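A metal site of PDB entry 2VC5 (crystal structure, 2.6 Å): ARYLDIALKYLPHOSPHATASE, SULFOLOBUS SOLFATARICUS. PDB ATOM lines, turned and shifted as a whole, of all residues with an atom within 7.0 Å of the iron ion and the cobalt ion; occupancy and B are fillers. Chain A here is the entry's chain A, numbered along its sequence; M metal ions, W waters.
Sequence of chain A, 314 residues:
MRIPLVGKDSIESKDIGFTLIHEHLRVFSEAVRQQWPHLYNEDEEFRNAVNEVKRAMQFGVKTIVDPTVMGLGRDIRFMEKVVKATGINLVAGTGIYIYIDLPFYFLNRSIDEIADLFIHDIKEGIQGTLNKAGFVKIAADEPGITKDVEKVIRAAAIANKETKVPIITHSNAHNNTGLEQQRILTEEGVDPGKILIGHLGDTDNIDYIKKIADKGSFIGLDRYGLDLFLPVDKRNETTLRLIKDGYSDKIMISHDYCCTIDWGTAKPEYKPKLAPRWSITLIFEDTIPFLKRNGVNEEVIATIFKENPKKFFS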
ATOM      1  N   HIS A  22      10.379 -19.637 -12.241  1.00  0.00           N
ATOM      2  CA  HIS A  22      11.460 -19.941 -13.183  1.00  0.00           C
ATOM      3  C   HIS A  22      11.998 -21.356 -12.982  1.00  0.00           C
ATOM      4  O   HIS A  22      12.940 -21.561 -12.216  1.00  0.00           O
ATOM      5  CB  HIS A  22      12.575 -18.896 -13.040  1.00  0.00           C
ATOM      6  CG  HIS A  22      13.498 -18.831 -14.217  1.00  0.00           C
ATOM      7  ND1 HIS A  22      13.701 -17.671 -14.935  1.00  0.00           N
ATOM      8  CD2 HIS A  22      14.290 -19.774 -14.777  1.00  0.00           C
ATOM      9  CE1 HIS A  22      14.577 -17.906 -15.902  1.00  0.00           C
ATOM     10  NE2 HIS A  22      14.953 -19.172 -15.830  1.00  0.00           N
ATOM     11  N   GLU A  23      11.402 -22.312 -13.694  1.00  0.00           N
ATOM     12  CA  GLU A  23      11.837 -23.719 -13.654  1.00  0.00           C
ATOM     13  C   GLU A  23      11.758 -24.338 -15.047  1.00  0.00           C
ATOM     14  O   GLU A  23      10.835 -24.040 -15.798  1.00  0.00           O
ATOM     15  CB  GLU A  23      10.961 -24.548 -12.695  1.00  0.00           C
ATOM     16  CG  GLU A  23      10.734 -23.943 -11.300  1.00  0.00           C
ATOM     17  CD  GLU A  23      11.978 -23.888 -10.443  1.00  0.00           C
ATOM     18  OE1 GLU A  23      12.010 -23.073  -9.498  1.00  0.00           O
ATOM     19  OE2 GLU A  23      12.939 -24.649 -10.704  1.00  0.00           O
ATOM     20  N   HIS A  24      12.709 -25.203 -15.372  1.00  0.00           N
ATOM     21  CA  HIS A  24      12.735 -25.850 -16.687  1.00  0.00           C
ATOM     22  C   HIS A  24      12.441 -27.342 -16.573  1.00  0.00           C
ATOM     23  O   HIS A  24      13.083 -28.055 -15.785  1.00  0.00           O
ATOM     24  CB  HIS A  24      14.093 -25.644 -17.357  1.00  0.00           C
ATOM     25  CG  HIS A  24      14.413 -24.217 -17.678  1.00  0.00           C
ATOM     26  ND1 HIS A  24      13.995 -23.601 -18.831  1.00  0.00           N
ATOM     27  CD2 HIS A  24      15.128 -23.290 -16.992  1.00  0.00           C
ATOM     28  CE1 HIS A  24      14.426 -22.347 -18.845  1.00  0.00           C
ATOM     29  NE2 HIS A  24      15.120 -22.138 -17.737  1.00  0.00           N
ATOM     30  N   VAL A  27      15.767 -28.797 -20.956  1.00  0.00           N
ATOM     31  CA  VAL A  27      16.394 -27.954 -21.982  1.00  0.00           C
ATOM     32  C   VAL A  27      17.364 -28.765 -22.839  1.00  0.00           C
ATOM     33  O   VAL A  27      17.983 -29.718 -22.360  1.00  0.00           O
ATOM     34  CB  VAL A  27      17.076 -26.659 -21.406  1.00  0.00           C
ATOM     35  CG1 VAL A  27      16.613 -26.356 -19.995  1.00  0.00           C
ATOM     36  CG2 VAL A  27      18.598 -26.736 -21.461  1.00  0.00           C
ATOM     37  N   PRO A  67      10.202 -21.027 -18.630  1.00  0.00           N
ATOM     38  CA  PRO A  67      10.731 -20.095 -19.622  1.00  0.00           C
ATOM     39  C   PRO A  67      11.667 -20.725 -20.659  1.00  0.00           C
ATOM     40  O   PRO A  67      12.550 -20.045 -21.193  1.00  0.00           O
ATOM     41  CB  PRO A  67      11.474 -19.073 -18.754  1.00  0.00           C
ATOM     42  CG  PRO A  67      11.892 -19.830 -17.527  1.00  0.00           C
ATOM     43  CD  PRO A  67      11.038 -21.075 -17.419  1.00  0.00           C
ATOM     44  N   THR A  68      11.468 -22.003 -20.940  1.00  0.00           N
ATOM     45  CA  THR A  68      12.143 -22.684 -22.040  1.00  0.00           C
ATOM     46  C   THR A  68      11.570 -22.137 -23.352  1.00  0.00           C
ATOM     47  O   THR A  68      10.387 -22.314 -23.647  1.00  0.00           O
ATOM     48  CB  THR A  68      11.940 -24.212 -21.994  1.00  0.00           C
ATOM     49  OG1 THR A  68      12.305 -24.698 -20.686  1.00  0.00           O
ATOM     50  CG2 THR A  68      12.798 -24.905 -23.031  1.00  0.00           C
ATOM     51  N   LEU A  72      16.558 -23.059 -26.241  1.00  0.00           N
ATOM     52  CA  LEU A  72      16.566 -23.948 -25.078  1.00  0.00           C
ATOM     53  C   LEU A  72      15.727 -25.215 -25.286  1.00  0.00           C
ATOM     54  O   LEU A  72      15.602 -26.043 -24.380  1.00  0.00           O
ATOM     55  CB  LEU A  72      16.100 -23.203 -23.809  1.00  0.00           C
ATOM     56  CG  LEU A  72      16.899 -22.006 -23.281  1.00  0.00           C
ATOM     57  CD1 LEU A  72      16.173 -21.391 -22.094  1.00  0.00           C
ATOM     58  CD2 LEU A  72      18.327 -22.389 -22.884  1.00  0.00           C
ATOM     59  N   TYR A  97      16.191 -17.149 -26.867  1.00  0.00           N
ATOM     60  CA  TYR A  97      17.296 -17.226 -25.926  1.00  0.00           C
ATOM     61  C   TYR A  97      18.632 -17.204 -26.674  1.00  0.00           C
ATOM     62  O   TYR A  97      19.045 -18.209 -27.266  1.00  0.00           O
ATOM     63  CB  TYR A  97      17.182 -18.504 -25.090  1.00  0.00           C
ATOM     64  CG  TYR A  97      18.160 -18.606 -23.945  1.00  0.00           C
ATOM     65  CD1 TYR A  97      19.438 -19.130 -24.138  1.00  0.00           C
ATOM     66  CD2 TYR A  97      17.802 -18.190 -22.662  1.00  0.00           C
ATOM     67  CE1 TYR A  97      20.346 -19.230 -23.086  1.00  0.00           C
ATOM     68  CE2 TYR A  97      18.697 -18.292 -21.603  1.00  0.00           C
ATOM     69  CZ  TYR A  97      19.960 -18.806 -21.825  1.00  0.00           C
ATOM     70  OH  TYR A  97      20.847 -18.911 -20.770  1.00  0.00           O
ATOM     71  N   TYR A  99      22.828 -15.153 -26.547  1.00  0.00           N
ATOM     72  CA  TYR A  99      23.785 -14.264 -25.880  1.00  0.00           C
ATOM     73  C   TYR A  99      24.474 -13.320 -26.864  1.00  0.00           C
ATOM     74  O   TYR A  99      24.902 -12.232 -26.476  1.00  0.00           O
ATOM     75  CB  TYR A  99      24.854 -15.040 -25.110  1.00  0.00           C
ATOM     76  CG  TYR A  99      24.383 -15.893 -23.945  1.00  0.00           C
ATOM     77  CD1 TYR A  99      23.096 -15.776 -23.415  1.00  0.00           C
ATOM     78  CD2 TYR A  99      25.258 -16.813 -23.339  1.00  0.00           C
ATOM     79  CE1 TYR A  99      22.682 -16.574 -22.344  1.00  0.00           C
ATOM     80  CE2 TYR A  99      24.854 -17.600 -22.277  1.00  0.00           C
ATOM     81  CZ  TYR A  99      23.566 -17.481 -21.779  1.00  0.00           C
ATOM     82  OH  TYR A  99      23.184 -18.263 -20.720  1.00  0.00           O
ATOM     83  N   KCX A 137      10.145 -14.532 -23.101  1.00  0.00           N
ATOM     84  CA  KCX A 137      11.467 -14.678 -22.497  1.00  0.00           C
ATOM     85  CB  KCX A 137      11.753 -16.151 -22.182  1.00  0.00           C
ATOM     86  CG  KCX A 137      12.637 -16.385 -20.957  1.00  0.00           C
ATOM     87  CD  KCX A 137      14.116 -16.257 -21.253  1.00  0.00           C
ATOM     88  CE  KCX A 137      14.951 -16.530 -20.009  1.00  0.00           C
ATOM     89  NZ  KCX A 137      14.980 -17.983 -19.645  1.00  0.00           N
ATOM     90  C   KCX A 137      12.563 -14.121 -23.407  1.00  0.00           C
ATOM     91  O   KCX A 137      12.636 -14.457 -24.586  1.00  0.00           O
ATOM     92  CX  KCX A 137      15.957 -18.501 -18.895  1.00  0.00           C
ATOM     93  OQ1 KCX A 137      16.878 -17.803 -18.452  1.00  0.00           O
ATOM     94  OQ2 KCX A 137      15.947 -19.711 -18.625  1.00  0.00           O
ATOM     95  N   ILE A 138      13.405 -13.270 -22.823  1.00  0.00           N
ATOM     96  CA  ILE A 138      14.586 -12.722 -23.514  1.00  0.00           C
ATOM     97  C   ILE A 138      15.840 -12.919 -22.659  1.00  0.00           C
ATOM     98  O   ILE A 138      15.740 -13.226 -21.472  1.00  0.00           O
ATOM     99  CB  ILE A 138      14.380 -11.229 -23.921  1.00  0.00           C
ATOM    100  CG1 ILE A 138      14.115 -10.339 -22.702  1.00  0.00           C
ATOM    101  CG2 ILE A 138      13.249 -11.087 -24.915  1.00  0.00           C
ATOM    102  CD1 ILE A 138      15.287  -9.491 -22.303  1.00  0.00           C
ATOM    103  N   ALA A 139      17.014 -12.765 -23.263  1.00  0.00           N
ATOM    104  CA  ALA A 139      18.278 -13.078 -22.582  1.00  0.00           C
ATOM    105  C   ALA A 139      19.434 -12.129 -22.919  1.00  0.00           C
ATOM    106  O   ALA A 139      19.436 -11.484 -23.965  1.00  0.00           O
ATOM    107  CB  ALA A 139      18.667 -14.521 -22.859  1.00  0.00           C
ATOM    108  N   ASP A 141      23.969 -11.945 -21.584  1.00  0.00           N
ATOM    109  CA  ASP A 141      24.993 -12.456 -20.687  1.00  0.00           C
ATOM    110  C   ASP A 141      26.309 -11.656 -20.755  1.00  0.00           C
ATOM    111  O   ASP A 141      26.278 -10.449 -20.998  1.00  0.00           O
ATOM    112  CB  ASP A 141      25.220 -13.953 -20.921  1.00  0.00           C
ATOM    113  CG  ASP A 141      25.390 -14.736 -19.625  1.00  0.00           C
ATOM    114  OD1 ASP A 141      26.370 -14.494 -18.897  1.00  0.00           O
ATOM    115  OD2 ASP A 141      24.526 -15.587 -19.329  1.00  0.00           O
ATOM    116  N   THR A 169      13.284 -12.219 -18.050  1.00  0.00           N
ATOM    117  CA  THR A 169      14.622 -12.065 -18.611  1.00  0.00           C
ATOM    118  C   THR A 169      15.633 -13.017 -17.980  1.00  0.00           C
ATOM    119  O   THR A 169      15.489 -13.418 -16.829  1.00  0.00           O
ATOM    120  CB  THR A 169      15.167 -10.632 -18.456  1.00  0.00           C
ATOM    121  OG1 THR A 169      15.614 -10.428 -17.108  1.00  0.00           O
ATOM    122  CG2 THR A 169      14.107  -9.591 -18.805  1.00  0.00           C
ATOM    123  N   HIS A 170      16.641 -13.356 -18.771  1.00  0.00           N
ATOM    124  CA  HIS A 170      17.878 -13.947 -18.288  1.00  0.00           C
ATOM    125  C   HIS A 170      18.903 -12.809 -18.367  1.00  0.00           C
ATOM    126  O   HIS A 170      18.930 -12.069 -19.353  1.00  0.00           O
ATOM    127  CB  HIS A 170      18.284 -15.107 -19.195  1.00  0.00           C
ATOM    128  CG  HIS A 170      19.678 -15.622 -18.954  1.00  0.00           C
ATOM    129  ND1 HIS A 170      19.927 -16.822 -18.314  1.00  0.00           N
ATOM    130  CD2 HIS A 170      20.887 -15.117 -19.292  1.00  0.00           C
ATOM    131  CE1 HIS A 170      21.233 -17.024 -18.261  1.00  0.00           C
ATOM    132  NE2 HIS A 170      21.838 -16.003 -18.846  1.00  0.00           N
ATOM    133  N   SER A 171      19.728 -12.672 -17.339  1.00  0.00           N
ATOM    134  CA  SER A 171      20.814 -11.683 -17.351  1.00  0.00           C
ATOM    135  C   SER A 171      22.040 -12.164 -16.585  1.00  0.00           C
ATOM    136  O   SER A 171      21.950 -13.093 -15.780  1.00  0.00           O
ATOM    137  CB  SER A 171      20.345 -10.332 -16.811  1.00  0.00           C
ATOM    138  OG  SER A 171      20.608 -10.209 -15.426  1.00  0.00           O
ATOM    139  N   GLY A 198      15.971 -11.372 -14.468  1.00  0.00           N
ATOM    140  CA  GLY A 198      16.410 -12.665 -13.967  1.00  0.00           C
ATOM    141  C   GLY A 198      17.831 -12.731 -13.445  1.00  0.00           C
ATOM    142  O   GLY A 198      18.693 -11.945 -13.830  1.00  0.00           O
ATOM    143  N   HIS A 199      18.045 -13.697 -12.549  1.00  0.00           N
ATOM    144  CA  HIS A 199      19.373 -14.095 -12.069  1.00  0.00           C
ATOM    145  C   HIS A 199      20.122 -13.033 -11.259  1.00  0.00           C
ATOM    146  O   HIS A 199      21.355 -13.029 -11.200  1.00  0.00           O
ATOM    147  CB  HIS A 199      20.223 -14.658 -13.215  1.00  0.00           C
ATOM    148  CG  HIS A 199      19.484 -15.617 -14.090  1.00  0.00           C
ATOM    149  ND1 HIS A 199      18.718 -16.645 -13.578  1.00  0.00           N
ATOM    150  CD2 HIS A 199      19.374 -15.711 -15.430  1.00  0.00           C
ATOM    151  CE1 HIS A 199      18.178 -17.326 -14.568  1.00  0.00           C
ATOM    152  NE2 HIS A 199      18.555 -16.776 -15.704  1.00  0.00           N
ATOM    153  N   ASP A 222      16.476 -16.233  -8.360  1.00  0.00           N
ATOM    154  CA  ASP A 222      15.807 -17.363  -9.010  1.00  0.00           C
ATOM    155  C   ASP A 222      16.677 -18.585  -9.325  1.00  0.00           C
ATOM    156  O   ASP A 222      16.246 -19.483 -10.057  1.00  0.00           O
ATOM    157  CB  ASP A 222      15.133 -16.868 -10.299  1.00  0.00           C
ATOM    158  CG  ASP A 222      16.073 -16.084 -11.205  1.00  0.00           C
ATOM    159  OD1 ASP A 222      15.594 -15.167 -11.895  1.00  0.00           O
ATOM    160  OD2 ASP A 222      17.292 -16.364 -11.208  1.00  0.00           O
ATOM    161  N   ARG A 223      17.885 -18.645  -8.768  1.00  0.00           N
ATOM    162  CA  ARG A 223      18.805 -19.752  -9.049  1.00  0.00           C
ATOM    163  C   ARG A 223      19.273 -20.512  -7.802  1.00  0.00           C
ATOM    164  O   ARG A 223      20.419 -20.966  -7.743  1.00  0.00           O
ATOM    165  CB  ARG A 223      20.003 -19.261  -9.866  1.00  0.00           C
ATOM    166  CG  ARG A 223      19.726 -19.115 -11.350  1.00  0.00           C
ATOM    167  CD  ARG A 223      20.981 -18.754 -12.104  1.00  0.00           C
ATOM    168  NE  ARG A 223      20.858 -19.053 -13.528  1.00  0.00           N
ATOM    169  CZ  ARG A 223      21.774 -18.767 -14.447  1.00  0.00           C
ATOM    170  NH1 ARG A 223      21.572 -19.090 -15.714  1.00  0.00           N
ATOM    171  NH2 ARG A 223      22.902 -18.165 -14.094  1.00  0.00           N
ATOM    172  N   ASP A 256      15.485 -22.280 -11.040  1.00  0.00           N
ATOM    173  CA  ASP A 256      16.043 -22.397 -12.398  1.00  0.00           C
ATOM    174  C   ASP A 256      16.468 -23.851 -12.670  1.00  0.00           C
ATOM    175  O   ASP A 256      17.288 -24.111 -13.546  1.00  0.00           O
ATOM    176  CB  ASP A 256      17.201 -21.417 -12.608  1.00  0.00           C
ATOM    177  CG  ASP A 256      17.566 -21.218 -14.076  1.00  0.00           C
ATOM    178  OD1 ASP A 256      18.673 -20.711 -14.346  1.00  0.00           O
ATOM    179  OD2 ASP A 256      16.753 -21.561 -14.962  1.00  0.00           O
ATOM    180  N   TYR A 257      15.894 -24.779 -11.913  1.00  0.00           N
ATOM    181  CA  TYR A 257      16.241 -26.186 -12.038  1.00  0.00           C
ATOM    182  C   TYR A 257      15.808 -26.775 -13.368  1.00  0.00           C
ATOM    183  O   TYR A 257      14.689 -26.543 -13.839  1.00  0.00           O
ATOM    184  CB  TYR A 257      15.692 -27.030 -10.884  1.00  0.00           C
ATOM    185  CG  TYR A 257      16.185 -28.471 -10.914  1.00  0.00           C
ATOM    186  CD1 TYR A 257      17.485 -28.785 -10.533  1.00  0.00           C
ATOM    187  CD2 TYR A 257      15.351 -29.503 -11.339  1.00  0.00           C
ATOM    188  CE1 TYR A 257      17.948 -30.098 -10.573  1.00  0.00           C
ATOM    189  CE2 TYR A 257      15.805 -30.819 -11.381  1.00  0.00           C
ATOM    190  CZ  TYR A 257      17.105 -31.110 -10.993  1.00  0.00           C
ATOM    191  OH  TYR A 257      17.554 -32.407 -11.040  1.00  0.00           O
ATOM    192  N   CYS A 258      16.717 -27.529 -13.975  1.00  0.00           N
ATOM    193  CA  CYS A 258      16.399 -28.298 -15.168  1.00  0.00           C
ATOM    194  C   CYS A 258      16.468 -29.764 -14.808  1.00  0.00           C
ATOM    195  O   CYS A 258      17.501 -30.248 -14.323  1.00  0.00           O
ATOM    196  CB  CYS A 258      17.385 -27.982 -16.292  1.00  0.00           C
ATOM    197  SG  CYS A 258      17.863 -26.242 -16.413  1.00  0.00           S
HETATM  198 FE    FE M   1      16.353 -20.561 -16.814  1.00  0.00          FE
HETATM  199 CO    CO M   2      18.557 -18.030 -17.383  1.00  0.00          CO
HETATM  200  O   HOH W   1      18.075 -19.628 -16.775  1.00  0.00           O
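Of the 23 residues printed, 4 come within 4 Å of the iron ion.
Water W1 is bound to the cobalt ion, 1.8 Å away. The cobalt ion is bound by OQ1 of KCX 137, 2.0 Å away. A ring nitrogen (ND1) of His 170 binds the cobalt ion, 2.1 Å away. The cobalt ion is bound by a ring nitrogen (NE2) of His 199 (2.1 Å).
N of His 170 sits at hydrogen-bond distance from O of Ile 138 (2.9 Å). N of Asp 256 lies within hydrogen-bond range of OE2 of Glu 23 (3.5 Å). The side-chain carboxylate (OD1) of Asp 256 is in salt-bridge range of the guanidinium group (NE) of Arg 223 (2.9 Å). A ring nitrogen (ND1) of His 24 sits at hydrogen-bond distance from the side-chain hydroxyl (OG1) of Thr 68 (2.7 Å). ND1 of His 199 is in hydrogen-bond range of OD2 of Asp 222 (2.8 Å). The side-chain carboxylate (OD2) of Asp 141 lies within hydrogen-bond range of a ring nitrogen (NE2) of His 170, 2.8 Å away. The side-chain hydroxyl of Tyr 99 lies within hydrogen-bond range of a ring nitrogen (NE2) of His 170, 3.2 Å away. The side-chain hydroxyl (OH) of Tyr 97 sits close to a ring nitrogen (ND1) of His 170, at 3.4 Å.
The iron ion is bound by water W1 (2.0 Å), OQ2 of KCX 137 (2.0 Å), OD2 of Asp 256 (2.1 Å), NE2 of His 22 (2.2 Å) and NE2 of His 24 (2.2 Å).
Merely in contact with the cobalt ion: Arg 223 (3.6 Å). Four residues have an atom within 4 Å of the cobalt ion: KCX 137, His 170, His 199 and Arg 223.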
